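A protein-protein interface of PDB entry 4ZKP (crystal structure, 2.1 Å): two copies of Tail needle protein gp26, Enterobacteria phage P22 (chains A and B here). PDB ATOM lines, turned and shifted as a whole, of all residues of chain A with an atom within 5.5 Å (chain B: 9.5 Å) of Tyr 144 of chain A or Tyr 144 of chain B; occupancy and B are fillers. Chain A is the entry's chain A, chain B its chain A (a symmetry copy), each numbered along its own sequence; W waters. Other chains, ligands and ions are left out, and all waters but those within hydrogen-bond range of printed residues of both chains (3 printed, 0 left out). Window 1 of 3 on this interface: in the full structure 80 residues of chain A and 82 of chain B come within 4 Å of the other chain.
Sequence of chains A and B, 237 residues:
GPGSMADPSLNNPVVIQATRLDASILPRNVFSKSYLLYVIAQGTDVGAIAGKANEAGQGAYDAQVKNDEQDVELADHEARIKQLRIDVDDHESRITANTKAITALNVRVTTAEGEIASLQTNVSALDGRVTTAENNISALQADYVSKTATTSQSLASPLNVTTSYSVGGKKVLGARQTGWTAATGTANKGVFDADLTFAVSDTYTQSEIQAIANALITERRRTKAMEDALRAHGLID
OD2 of Asp 143 of chain A lies within hydrogen-bond range of OG of Ser 146 of chain B.
The side-chain carboxylate (OD2) of Asp 143 of chain A sits at hydrogen-bond distance from the side-chain hydroxyl (OH) of Tyr 144 of chain B, at 2.5 Å.
The backbone NH (N) of Val 145 of chain A is in hydrogen-bond range of the backbone carbonyl oxygen (O) of Val 145 of chain B (3.3 Å).
The side-chain carboxylate of Asp 143 of chain A lies within hydrogen-bond range of the side-chain hydroxyl of Thr 148 of chain B (2.5 Å).
O of Asp 143 of chain A sits at hydrogen-bond distance from N of Lys 147 of chain B.
N of Ala 149 of chain B is in hydrogen-bond range of OG of Ser 146 of chain B (3.0 Å).
O of Ser 146 of chain B lies within hydrogen-bond range of NE2 of Gln 153 of chain B (2.8 Å).
The backbone carbonyl oxygen (O) of Ser 146 of chain A lies within hydrogen-bond range of the side-chain amide nitrogen (NE2) of Gln 153 of chain A (2.8 Å).
The side-chain hydroxyl (OG) of Ser 146 of chain B is in hydrogen-bond range of the backbone NH (N) of Thr 148 of chain B (3.1 Å).
Among the printed residues, pairs that only touch across the chains: Leu 140 of chain A with Tyr 144 of chain B (3.7 Å), Asp 143 of chain A with Val 145 of chain B (3.7 Å), Tyr 144 of chain A with Tyr 144 of chain B (3.8 Å), Tyr 144 of chain A with Val 145 of chain B (3.7 Å), Tyr 144 of chain A with Lys 147 of chain B (3.1 Å) and Gln 153 of chain A with Lys 147 of chain B (3.8 Å).
Tyr 144 of chain A touches just these residues of chain B: Tyr 144, Val 145 and Lys 147.
Tyr 144 of chain B touches just these residues of chain A: Leu 140 (3.7 Å), Asp 143 (2.5 Å) and Tyr 144 (3.8 Å).
Of the printed residues of chain B, Asp 143 of chain A touches Tyr 144, Val 145, Ser 146, Lys 147 and Thr 148.
Of the printed residues of chain A, Val 145 of chain B touches Asp 143, Tyr 144 and Val 145.
Printed residues of chain B within 4 Å of Gln 153 of chain A: Lys 147.
Printed residues of chain B within 4 Å of Leu 140 of chain A: Tyr 144 (3.7 Å).
The nearest residue of chain B that does not touch Tyr 144 of chain A is Ser 146 of chain B (5.2 Å).
Printed residues of chain A that touch a printed residue of chain B: Leu 140, Asp 143, Tyr 144, Val 145 and Gln 153.
Hydrophobic or aromatic side chains of chain A that line the printed part of chain B: Leu 140, Tyr 144 and Val 145.
Hydrophobic or aromatic side chains of chain B within 4 Å of the printed part of chain A: Tyr 144 and Val 145.
Among the printed residues, no Asp or Glu carboxylate lies within 4 Å of a Lys or Arg side-chain nitrogen of the other chain.
Asp 143 of chain A touches Val 145 of chain B, but with the chains exchanged Val 145 of chain A does not touch Asp 143 of chain B (8.7 Å).
Tyr 144 of chain A touches Val 145 of chain B, but with the chains exchanged Val 145 of chain A does not touch Tyr 144 of chain B (5.1 Å).
Tyr 144 of chain A touches Lys 147 of chain B, but with the chains exchanged Lys 147 of chain A does not touch Tyr 144 of chain B (9.8 Å).
Gln 153 of chain A touches Lys 147 of chain B, but with the chains exchanged Lys 147 of chain A does not touch Gln 153 of chain B (13.5 Å).
Water W1 lies within hydrogen-bond range of NZ of Lys 147 of chain B and OE1 of Gln 153 of chain A.
Water W2 lies within hydrogen-bond range of O of Tyr 144 of chain A (2.9 Å), O of Gln 141 of chain A (2.9 Å) and NZ of Lys 147 of chain B (3.0 Å).
Water W3 lies within hydrogen-bond range of the backbone NH of Val 145 of chain A (3.1 Å) and the backbone NH of Val 145 of chain B (3.1 Å).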
ATOM      1  N   ALA A 139     -14.171 -16.799  -1.288  1.00  0.00           N
ATOM      2  CA  ALA A 139     -15.381 -16.882  -2.096  1.00  0.00           C
ATOM      3  C   ALA A 139     -15.601 -18.310  -2.586  1.00  0.00           C
ATOM      4  O   ALA A 139     -16.725 -18.809  -2.593  1.00  0.00           O
ATOM      5  CB  ALA A 139     -15.305 -15.919  -3.270  1.00  0.00           C
ATOM      6  N   LEU A 140     -14.515 -18.959  -2.996  1.00  0.00           N
ATOM      7  CA  LEU A 140     -14.562 -20.341  -3.463  1.00  0.00           C
ATOM      8  C   LEU A 140     -14.953 -21.302  -2.346  1.00  0.00           C
ATOM      9  O   LEU A 140     -15.802 -22.172  -2.535  1.00  0.00           O
ATOM     10  CB  LEU A 140     -13.213 -20.751  -4.058  1.00  0.00           C
ATOM     11  CG  LEU A 140     -12.934 -20.269  -5.482  1.00  0.00           C
ATOM     12  CD1 LEU A 140     -11.454 -20.389  -5.812  1.00  0.00           C
ATOM     13  CD2 LEU A 140     -13.774 -21.047  -6.484  1.00  0.00           C
ATOM     14  N   GLN A 141     -14.316 -21.143  -1.188  1.00  0.00           N
ATOM     15  CA  GLN A 141     -14.546 -22.008  -0.033  1.00  0.00           C
ATOM     16  C   GLN A 141     -16.022 -22.084   0.351  1.00  0.00           C
ATOM     17  O   GLN A 141     -16.514 -23.135   0.760  1.00  0.00           O
ATOM     18  CB  GLN A 141     -13.730 -21.517   1.165  1.00  0.00           C
ATOM     19  CG  GLN A 141     -12.250 -21.857   1.101  1.00  0.00           C
ATOM     20  CD  GLN A 141     -11.460 -21.227   2.232  1.00  0.00           C
ATOM     21  OE1 GLN A 141     -11.806 -20.152   2.722  1.00  0.00           O
ATOM     22  NE2 GLN A 141     -10.392 -21.894   2.652  1.00  0.00           N
ATOM     23  N   ALA A 142     -16.719 -20.961   0.220  1.00  0.00           N
ATOM     24  CA  ALA A 142     -18.123 -20.877   0.602  1.00  0.00           C
ATOM     25  C   ALA A 142     -19.054 -21.347  -0.514  1.00  0.00           C
ATOM     26  O   ALA A 142     -20.194 -21.730  -0.257  1.00  0.00           O
ATOM     27  CB  ALA A 142     -18.469 -19.452   1.005  1.00  0.00           C
ATOM     28  N   ASP A 143     -18.564 -21.316  -1.749  1.00  0.00           N
ATOM     29  CA  ASP A 143     -19.427 -21.511  -2.909  1.00  0.00           C
ATOM     30  C   ASP A 143     -19.235 -22.853  -3.623  1.00  0.00           C
ATOM     31  O   ASP A 143     -20.074 -23.250  -4.432  1.00  0.00           O
ATOM     32  CB  ASP A 143     -19.201 -20.367  -3.902  1.00  0.00           C
ATOM     33  CG  ASP A 143     -20.276 -20.296  -4.967  1.00  0.00           C
ATOM     34  OD1 ASP A 143     -21.471 -20.358  -4.609  1.00  0.00           O
ATOM     35  OD2 ASP A 143     -19.924 -20.173  -6.158  1.00  0.00           O
ATOM     36  N   TYR A 144     -18.144 -23.554  -3.329  1.00  0.00           N
ATOM     37  CA  TYR A 144     -17.812 -24.761  -4.085  1.00  0.00           C
ATOM     38  C   TYR A 144     -18.517 -26.000  -3.540  1.00  0.00           C
ATOM     39  O   TYR A 144     -18.869 -26.063  -2.363  1.00  0.00           O
ATOM     40  CB  TYR A 144     -16.298 -24.986  -4.097  1.00  0.00           C
ATOM     41  CG  TYR A 144     -15.773 -25.788  -2.926  1.00  0.00           C
ATOM     42  CD1 TYR A 144     -15.676 -25.228  -1.659  1.00  0.00           C
ATOM     43  CD2 TYR A 144     -15.360 -27.103  -3.095  1.00  0.00           C
ATOM     44  CE1 TYR A 144     -15.192 -25.962  -0.590  1.00  0.00           C
ATOM     45  CE2 TYR A 144     -14.875 -27.843  -2.035  1.00  0.00           C
ATOM     46  CZ  TYR A 144     -14.792 -27.268  -0.785  1.00  0.00           C
ATOM     47  OH  TYR A 144     -14.309 -28.003   0.273  1.00  0.00           O
ATOM     48  N   VAL A 145     -18.702 -26.992  -4.406  1.00  0.00           N
ATOM     49  CA  VAL A 145     -19.339 -28.246  -4.026  1.00  0.00           C
ATOM     50  C   VAL A 145     -18.275 -29.256  -3.614  1.00  0.00           C
ATOM     51  O   VAL A 145     -17.369 -29.567  -4.387  1.00  0.00           O
ATOM     52  CB  VAL A 145     -20.210 -28.798  -5.168  1.00  0.00           C
ATOM     53  CG1 VAL A 145     -20.755 -30.171  -4.806  1.00  0.00           C
ATOM     54  CG2 VAL A 145     -21.342 -27.834  -5.480  1.00  0.00           C
ATOM     55  N   SER A 146     -18.395 -29.764  -2.392  1.00  0.00           N
ATOM     56  CA  SER A 146     -17.368 -30.618  -1.800  1.00  0.00           C
ATOM     57  C   SER A 146     -17.622 -32.106  -2.032  1.00  0.00           C
ATOM     58  O   SER A 146     -18.760 -32.572  -1.973  1.00  0.00           O
ATOM     59  CB  SER A 146     -17.263 -30.343  -0.299  1.00  0.00           C
ATOM     60  OG  SER A 146     -16.513 -31.352   0.351  1.00  0.00           O
ATOM     61  N   LYS A 147     -16.547 -32.842  -2.301  1.00  0.00           N
ATOM     62  CA  LYS A 147     -16.619 -34.287  -2.491  1.00  0.00           C
ATOM     63  C   LYS A 147     -16.728 -35.033  -1.165  1.00  0.00           C
ATOM     64  O   LYS A 147     -17.153 -36.186  -1.127  1.00  0.00           O
ATOM     65  CB  LYS A 147     -15.380 -34.788  -3.239  1.00  0.00           C
ATOM     66  CG  LYS A 147     -15.259 -34.337  -4.682  1.00  0.00           C
ATOM     67  CD  LYS A 147     -14.121 -35.082  -5.367  1.00  0.00           C
ATOM     68  CE  LYS A 147     -13.844 -34.538  -6.756  1.00  0.00           C
ATOM     69  NZ  LYS A 147     -12.632 -35.166  -7.356  1.00  0.00           N
ATOM     70  N   GLN A 153     -25.924 -30.817   0.068  1.00  0.00           N
ATOM     71  CA  GLN A 153     -25.533 -29.596  -0.623  1.00  0.00           C
ATOM     72  C   GLN A 153     -26.546 -29.266  -1.710  1.00  0.00           C
ATOM     73  O   GLN A 153     -27.068 -30.158  -2.377  1.00  0.00           O
ATOM     74  CB  GLN A 153     -24.131 -29.744  -1.220  1.00  0.00           C
ATOM     75  CG  GLN A 153     -23.159 -30.501  -0.326  1.00  0.00           C
ATOM     76  CD  GLN A 153     -21.767 -30.599  -0.921  1.00  0.00           C
ATOM     77  OE1 GLN A 153     -21.114 -29.587  -1.172  1.00  0.00           O
ATOM     78  NE2 GLN A 153     -21.307 -31.825  -1.150  1.00  0.00           N
ATOM     79  N   ASN B 136      -3.638 -21.091 -10.189  1.00  0.00           N
ATOM     80  CA  ASN B 136      -4.394 -22.205  -9.632  1.00  0.00           C
ATOM     81  C   ASN B 136      -5.809 -21.755  -9.284  1.00  0.00           C
ATOM     82  O   ASN B 136      -6.765 -22.521  -9.414  1.00  0.00           O
ATOM     83  CB  ASN B 136      -3.699 -22.769  -8.391  1.00  0.00           C
ATOM     84  CG  ASN B 136      -2.510 -23.646  -8.736  1.00  0.00           C
ATOM     85  OD1 ASN B 136      -2.456 -24.244  -9.811  1.00  0.00           O
ATOM     86  ND2 ASN B 136      -1.552 -23.729  -7.820  1.00  0.00           N
ATOM     87  N   ILE B 137      -5.930 -20.508  -8.844  1.00  0.00           N
ATOM     88  CA  ILE B 137      -7.224 -19.933  -8.502  1.00  0.00           C
ATOM     89  C   ILE B 137      -8.053 -19.725  -9.765  1.00  0.00           C
ATOM     90  O   ILE B 137      -9.245 -20.034  -9.793  1.00  0.00           O
ATOM     91  CB  ILE B 137      -7.056 -18.610  -7.729  1.00  0.00           C
ATOM     92  CG1 ILE B 137      -6.493 -18.876  -6.332  1.00  0.00           C
ATOM     93  CG2 ILE B 137      -8.381 -17.865  -7.637  1.00  0.00           C
ATOM     94  CD1 ILE B 137      -6.236 -17.621  -5.527  1.00  0.00           C
ATOM     95  N   SER B 138      -7.412 -19.211 -10.809  1.00  0.00           N
ATOM     96  CA  SER B 138      -8.081 -18.958 -12.081  1.00  0.00           C
ATOM     97  C   SER B 138      -8.603 -20.247 -12.704  1.00  0.00           C
ATOM     98  O   SER B 138      -9.686 -20.267 -13.289  1.00  0.00           O
ATOM     99  CB  SER B 138      -7.132 -18.253 -13.052  1.00  0.00           C
ATOM    100  OG  SER B 138      -7.083 -16.861 -12.797  1.00  0.00           O
ATOM    101  N   ALA B 139      -7.829 -21.321 -12.576  1.00  0.00           N
ATOM    102  CA  ALA B 139      -8.232 -22.622 -13.094  1.00  0.00           C
ATOM    103  C   ALA B 139      -9.445 -23.150 -12.334  1.00  0.00           C
ATOM    104  O   ALA B 139     -10.366 -23.710 -12.925  1.00  0.00           O
ATOM    105  CB  ALA B 139      -7.079 -23.608 -13.012  1.00  0.00           C
ATOM    106  N   LEU B 140      -9.433 -22.964 -11.018  1.00  0.00           N
ATOM    107  CA  LEU B 140     -10.537 -23.386 -10.159  1.00  0.00           C
ATOM    108  C   LEU B 140     -11.812 -22.604 -10.454  1.00  0.00           C
ATOM    109  O   LEU B 140     -12.890 -23.185 -10.575  1.00  0.00           O
ATOM    110  CB  LEU B 140     -10.157 -23.232  -8.685  1.00  0.00           C
ATOM    111  CG  LEU B 140      -9.271 -24.332  -8.102  1.00  0.00           C
ATOM    112  CD1 LEU B 140      -8.648 -23.885  -6.788  1.00  0.00           C
ATOM    113  CD2 LEU B 140     -10.067 -25.615  -7.911  1.00  0.00           C
ATOM    114  N   GLN B 141     -11.679 -21.284 -10.555  1.00  0.00           N
ATOM    115  CA  GLN B 141     -12.811 -20.391 -10.793  1.00  0.00           C
ATOM    116  C   GLN B 141     -13.614 -20.788 -12.030  1.00  0.00           C
ATOM    117  O   GLN B 141     -14.839 -20.671 -12.049  1.00  0.00           O
ATOM    118  CB  GLN B 141     -12.322 -18.948 -10.943  1.00  0.00           C
ATOM    119  CG  GLN B 141     -11.954 -18.268  -9.635  1.00  0.00           C
ATOM    120  CD  GLN B 141     -11.340 -16.897  -9.844  1.00  0.00           C
ATOM    121  OE1 GLN B 141     -10.679 -16.648 -10.853  1.00  0.00           O
ATOM    122  NE2 GLN B 141     -11.554 -16.001  -8.889  1.00  0.00           N
ATOM    123  N   ALA B 142     -12.913 -21.253 -13.058  1.00  0.00           N
ATOM    124  CA  ALA B 142     -13.546 -21.617 -14.319  1.00  0.00           C
ATOM    125  C   ALA B 142     -14.089 -23.045 -14.302  1.00  0.00           C
ATOM    126  O   ALA B 142     -14.981 -23.386 -15.077  1.00  0.00           O
ATOM    127  CB  ALA B 142     -12.563 -21.446 -15.465  1.00  0.00           C
ATOM    128  N   ASP B 143     -13.546 -23.876 -13.416  1.00  0.00           N
ATOM    129  CA  ASP B 143     -13.808 -25.309 -13.467  1.00  0.00           C
ATOM    130  C   ASP B 143     -14.712 -25.828 -12.343  1.00  0.00           C
ATOM    131  O   ASP B 143     -15.225 -26.944 -12.426  1.00  0.00           O
ATOM    132  CB  ASP B 143     -12.477 -26.066 -13.440  1.00  0.00           C
ATOM    133  CG  ASP B 143     -12.624 -27.524 -13.824  1.00  0.00           C
ATOM    134  OD1 ASP B 143     -13.287 -27.806 -14.844  1.00  0.00           O
ATOM    135  OD2 ASP B 143     -12.074 -28.384 -13.107  1.00  0.00           O
ATOM    136  N   TYR B 144     -14.915 -25.029 -11.300  1.00  0.00           N
ATOM    137  CA  TYR B 144     -15.631 -25.514 -10.121  1.00  0.00           C
ATOM    138  C   TYR B 144     -17.145 -25.383 -10.267  1.00  0.00           C
ATOM    139  O   TYR B 144     -17.641 -24.536 -11.007  1.00  0.00           O
ATOM    140  CB  TYR B 144     -15.162 -24.773  -8.866  1.00  0.00           C
ATOM    141  CG  TYR B 144     -15.913 -23.492  -8.576  1.00  0.00           C
ATOM    142  CD1 TYR B 144     -15.696 -22.346  -9.331  1.00  0.00           C
ATOM    143  CD2 TYR B 144     -16.831 -23.427  -7.536  1.00  0.00           C
ATOM    144  CE1 TYR B 144     -16.380 -21.174  -9.062  1.00  0.00           C
ATOM    145  CE2 TYR B 144     -17.518 -22.262  -7.259  1.00  0.00           C
ATOM    146  CZ  TYR B 144     -17.290 -21.138  -8.024  1.00  0.00           C
ATOM    147  OH  TYR B 144     -17.973 -19.976  -7.750  1.00  0.00           O
ATOM    148  N   VAL B 145     -17.873 -26.223  -9.536  1.00  0.00           N
ATOM    149  CA  VAL B 145     -19.330 -26.203  -9.551  1.00  0.00           C
ATOM    150  C   VAL B 145     -19.841 -25.312  -8.424  1.00  0.00           C
ATOM    151  O   VAL B 145     -19.526 -25.532  -7.256  1.00  0.00           O
ATOM    152  CB  VAL B 145     -19.909 -27.623  -9.436  1.00  0.00           C
ATOM    153  CG1 VAL B 145     -21.425 -27.571  -9.315  1.00  0.00           C
ATOM    154  CG2 VAL B 145     -19.492 -28.460 -10.634  1.00  0.00           C
ATOM    155  N   SER B 146     -20.631 -24.307  -8.787  1.00  0.00           N
ATOM    156  CA  SER B 146     -21.067 -23.280  -7.845  1.00  0.00           C
ATOM    157  C   SER B 146     -22.410 -23.600  -7.191  1.00  0.00           C
ATOM    158  O   SER B 146     -23.325 -24.110  -7.838  1.00  0.00           O
ATOM    159  CB  SER B 146     -21.149 -21.926  -8.551  1.00  0.00           C
ATOM    160  OG  SER B 146     -21.854 -20.984  -7.764  1.00  0.00           O
ATOM    161  N   LYS B 147     -22.513 -23.297  -5.900  1.00  0.00           N
ATOM    162  CA  LYS B 147     -23.749 -23.490  -5.149  1.00  0.00           C
ATOM    163  C   LYS B 147     -24.765 -22.389  -5.431  1.00  0.00           C
ATOM    164  O   LYS B 147     -25.959 -22.560  -5.190  1.00  0.00           O
ATOM    165  CB  LYS B 147     -23.459 -23.523  -3.646  1.00  0.00           C
ATOM    166  CG  LYS B 147     -22.664 -24.719  -3.158  1.00  0.00           C
ATOM    167  CD  LYS B 147     -22.645 -24.746  -1.636  1.00  0.00           C
ATOM    168  CE  LYS B 147     -21.714 -25.818  -1.101  1.00  0.00           C
ATOM    169  NZ  LYS B 147     -21.582 -25.734   0.382  1.00  0.00           N
ATOM    170  N   THR B 148     -24.286 -21.258  -5.941  1.00  0.00           N
ATOM    171  CA  THR B 148     -25.123 -20.070  -6.081  1.00  0.00           C
ATOM    172  C   THR B 148     -25.443 -19.705  -7.527  1.00  0.00           C
ATOM    173  O   THR B 148     -26.388 -18.959  -7.784  1.00  0.00           O
ATOM    174  CB  THR B 148     -24.468 -18.849  -5.407  1.00  0.00           C
ATOM    175  OG1 THR B 148     -23.086 -18.779  -5.775  1.00  0.00           O
ATOM    176  CG2 THR B 148     -24.580 -18.958  -3.895  1.00  0.00           C
ATOM    177  N   ALA B 149     -24.649 -20.213  -8.465  1.00  0.00           N
ATOM    178  CA  ALA B 149     -24.877 -19.946  -9.883  1.00  0.00           C
ATOM    179  C   ALA B 149     -26.272 -20.404 -10.293  1.00  0.00           C
ATOM    180  O   ALA B 149     -26.753 -21.435  -9.829  1.00  0.00           O
ATOM    181  CB  ALA B 149     -23.820 -20.633 -10.732  1.00  0.00           C
ATOM    182  N   THR B 151     -27.362 -20.247 -13.777  1.00  0.00           N
ATOM    183  CA  THR B 151     -27.276 -20.845 -15.102  1.00  0.00           C
ATOM    184  C   THR B 151     -26.914 -22.318 -14.956  1.00  0.00           C
ATOM    185  O   THR B 151     -26.054 -22.669 -14.146  1.00  0.00           O
ATOM    186  CB  THR B 151     -26.235 -20.128 -15.988  1.00  0.00           C
ATOM    187  OG1 THR B 151     -26.634 -18.767 -16.190  1.00  0.00           O
ATOM    188  CG2 THR B 151     -26.109 -20.814 -17.340  1.00  0.00           C
ATOM    189  N   SER B 152     -27.587 -23.174 -15.724  1.00  0.00           N
ATOM    190  CA  SER B 152     -27.368 -24.616 -15.661  1.00  0.00           C
ATOM    191  C   SER B 152     -25.894 -24.975 -15.812  1.00  0.00           C
ATOM    192  O   SER B 152     -25.192 -24.428 -16.664  1.00  0.00           O
ATOM    193  CB  SER B 152     -28.187 -25.325 -16.742  1.00  0.00           C
ATOM    194  OG  SER B 152     -27.680 -26.623 -16.995  1.00  0.00           O
ATOM    195  N   GLN B 153     -25.430 -25.897 -14.976  1.00  0.00           N
ATOM    196  CA  GLN B 153     -24.033 -26.310 -14.994  1.00  0.00           C
ATOM    197  C   GLN B 153     -23.924 -27.757 -15.452  1.00  0.00           C
ATOM    198  O   GLN B 153     -24.762 -28.591 -15.109  1.00  0.00           O
ATOM    199  CB  GLN B 153     -23.403 -26.132 -13.610  1.00  0.00           C
ATOM    200  CG  GLN B 153     -23.853 -24.871 -12.887  1.00  0.00           C
ATOM    201  CD  GLN B 153     -23.185 -24.697 -11.537  1.00  0.00           C
ATOM    202  OE1 GLN B 153     -21.963 -24.596 -11.444  1.00  0.00           O
ATOM    203  NE2 GLN B 153     -23.989 -24.662 -10.480  1.00  0.00           N
ATOM    204  N   SER B 154     -22.885 -28.052 -16.228  1.00  0.00           N
ATOM    205  CA  SER B 154     -22.741 -29.369 -16.833  1.00  0.00           C
ATOM    206  C   SER B 154     -21.419 -30.037 -16.467  1.00  0.00           C
ATOM    207  O   SER B 154     -20.365 -29.400 -16.478  1.00  0.00           O
ATOM    208  CB  SER B 154     -22.864 -29.265 -18.355  1.00  0.00           C
ATOM    209  OG  SER B 154     -22.673 -30.526 -18.971  1.00  0.00           O
ATOM    210  N   LEU B 155     -21.486 -31.323 -16.139  1.00  0.00           N
ATOM    211  CA  LEU B 155     -20.288 -32.112 -15.873  1.00  0.00           C
ATOM    212  C   LEU B 155     -19.936 -32.975 -17.080  1.00  0.00           C
ATOM    213  O   LEU B 155     -20.817 -33.411 -17.820  1.00  0.00           O
ATOM    214  CB  LEU B 155     -20.477 -32.994 -14.637  1.00  0.00           C
ATOM    215  CG  LEU B 155     -21.080 -32.355 -13.386  1.00  0.00           C
ATOM    216  CD1 LEU B 155     -21.109 -33.356 -12.242  1.00  0.00           C
ATOM    217  CD2 LEU B 155     -20.300 -31.114 -12.994  1.00  0.00           C
HETATM  218  O   HOH W   1     -20.322 -28.030   0.840  1.00  0.00           O
HETATM  219  O   HOH W   2     -18.620 -25.064   0.298  1.00  0.00           O
HETATM  220  O   HOH W   3     -17.092 -27.612  -6.928  1.00  0.00           O
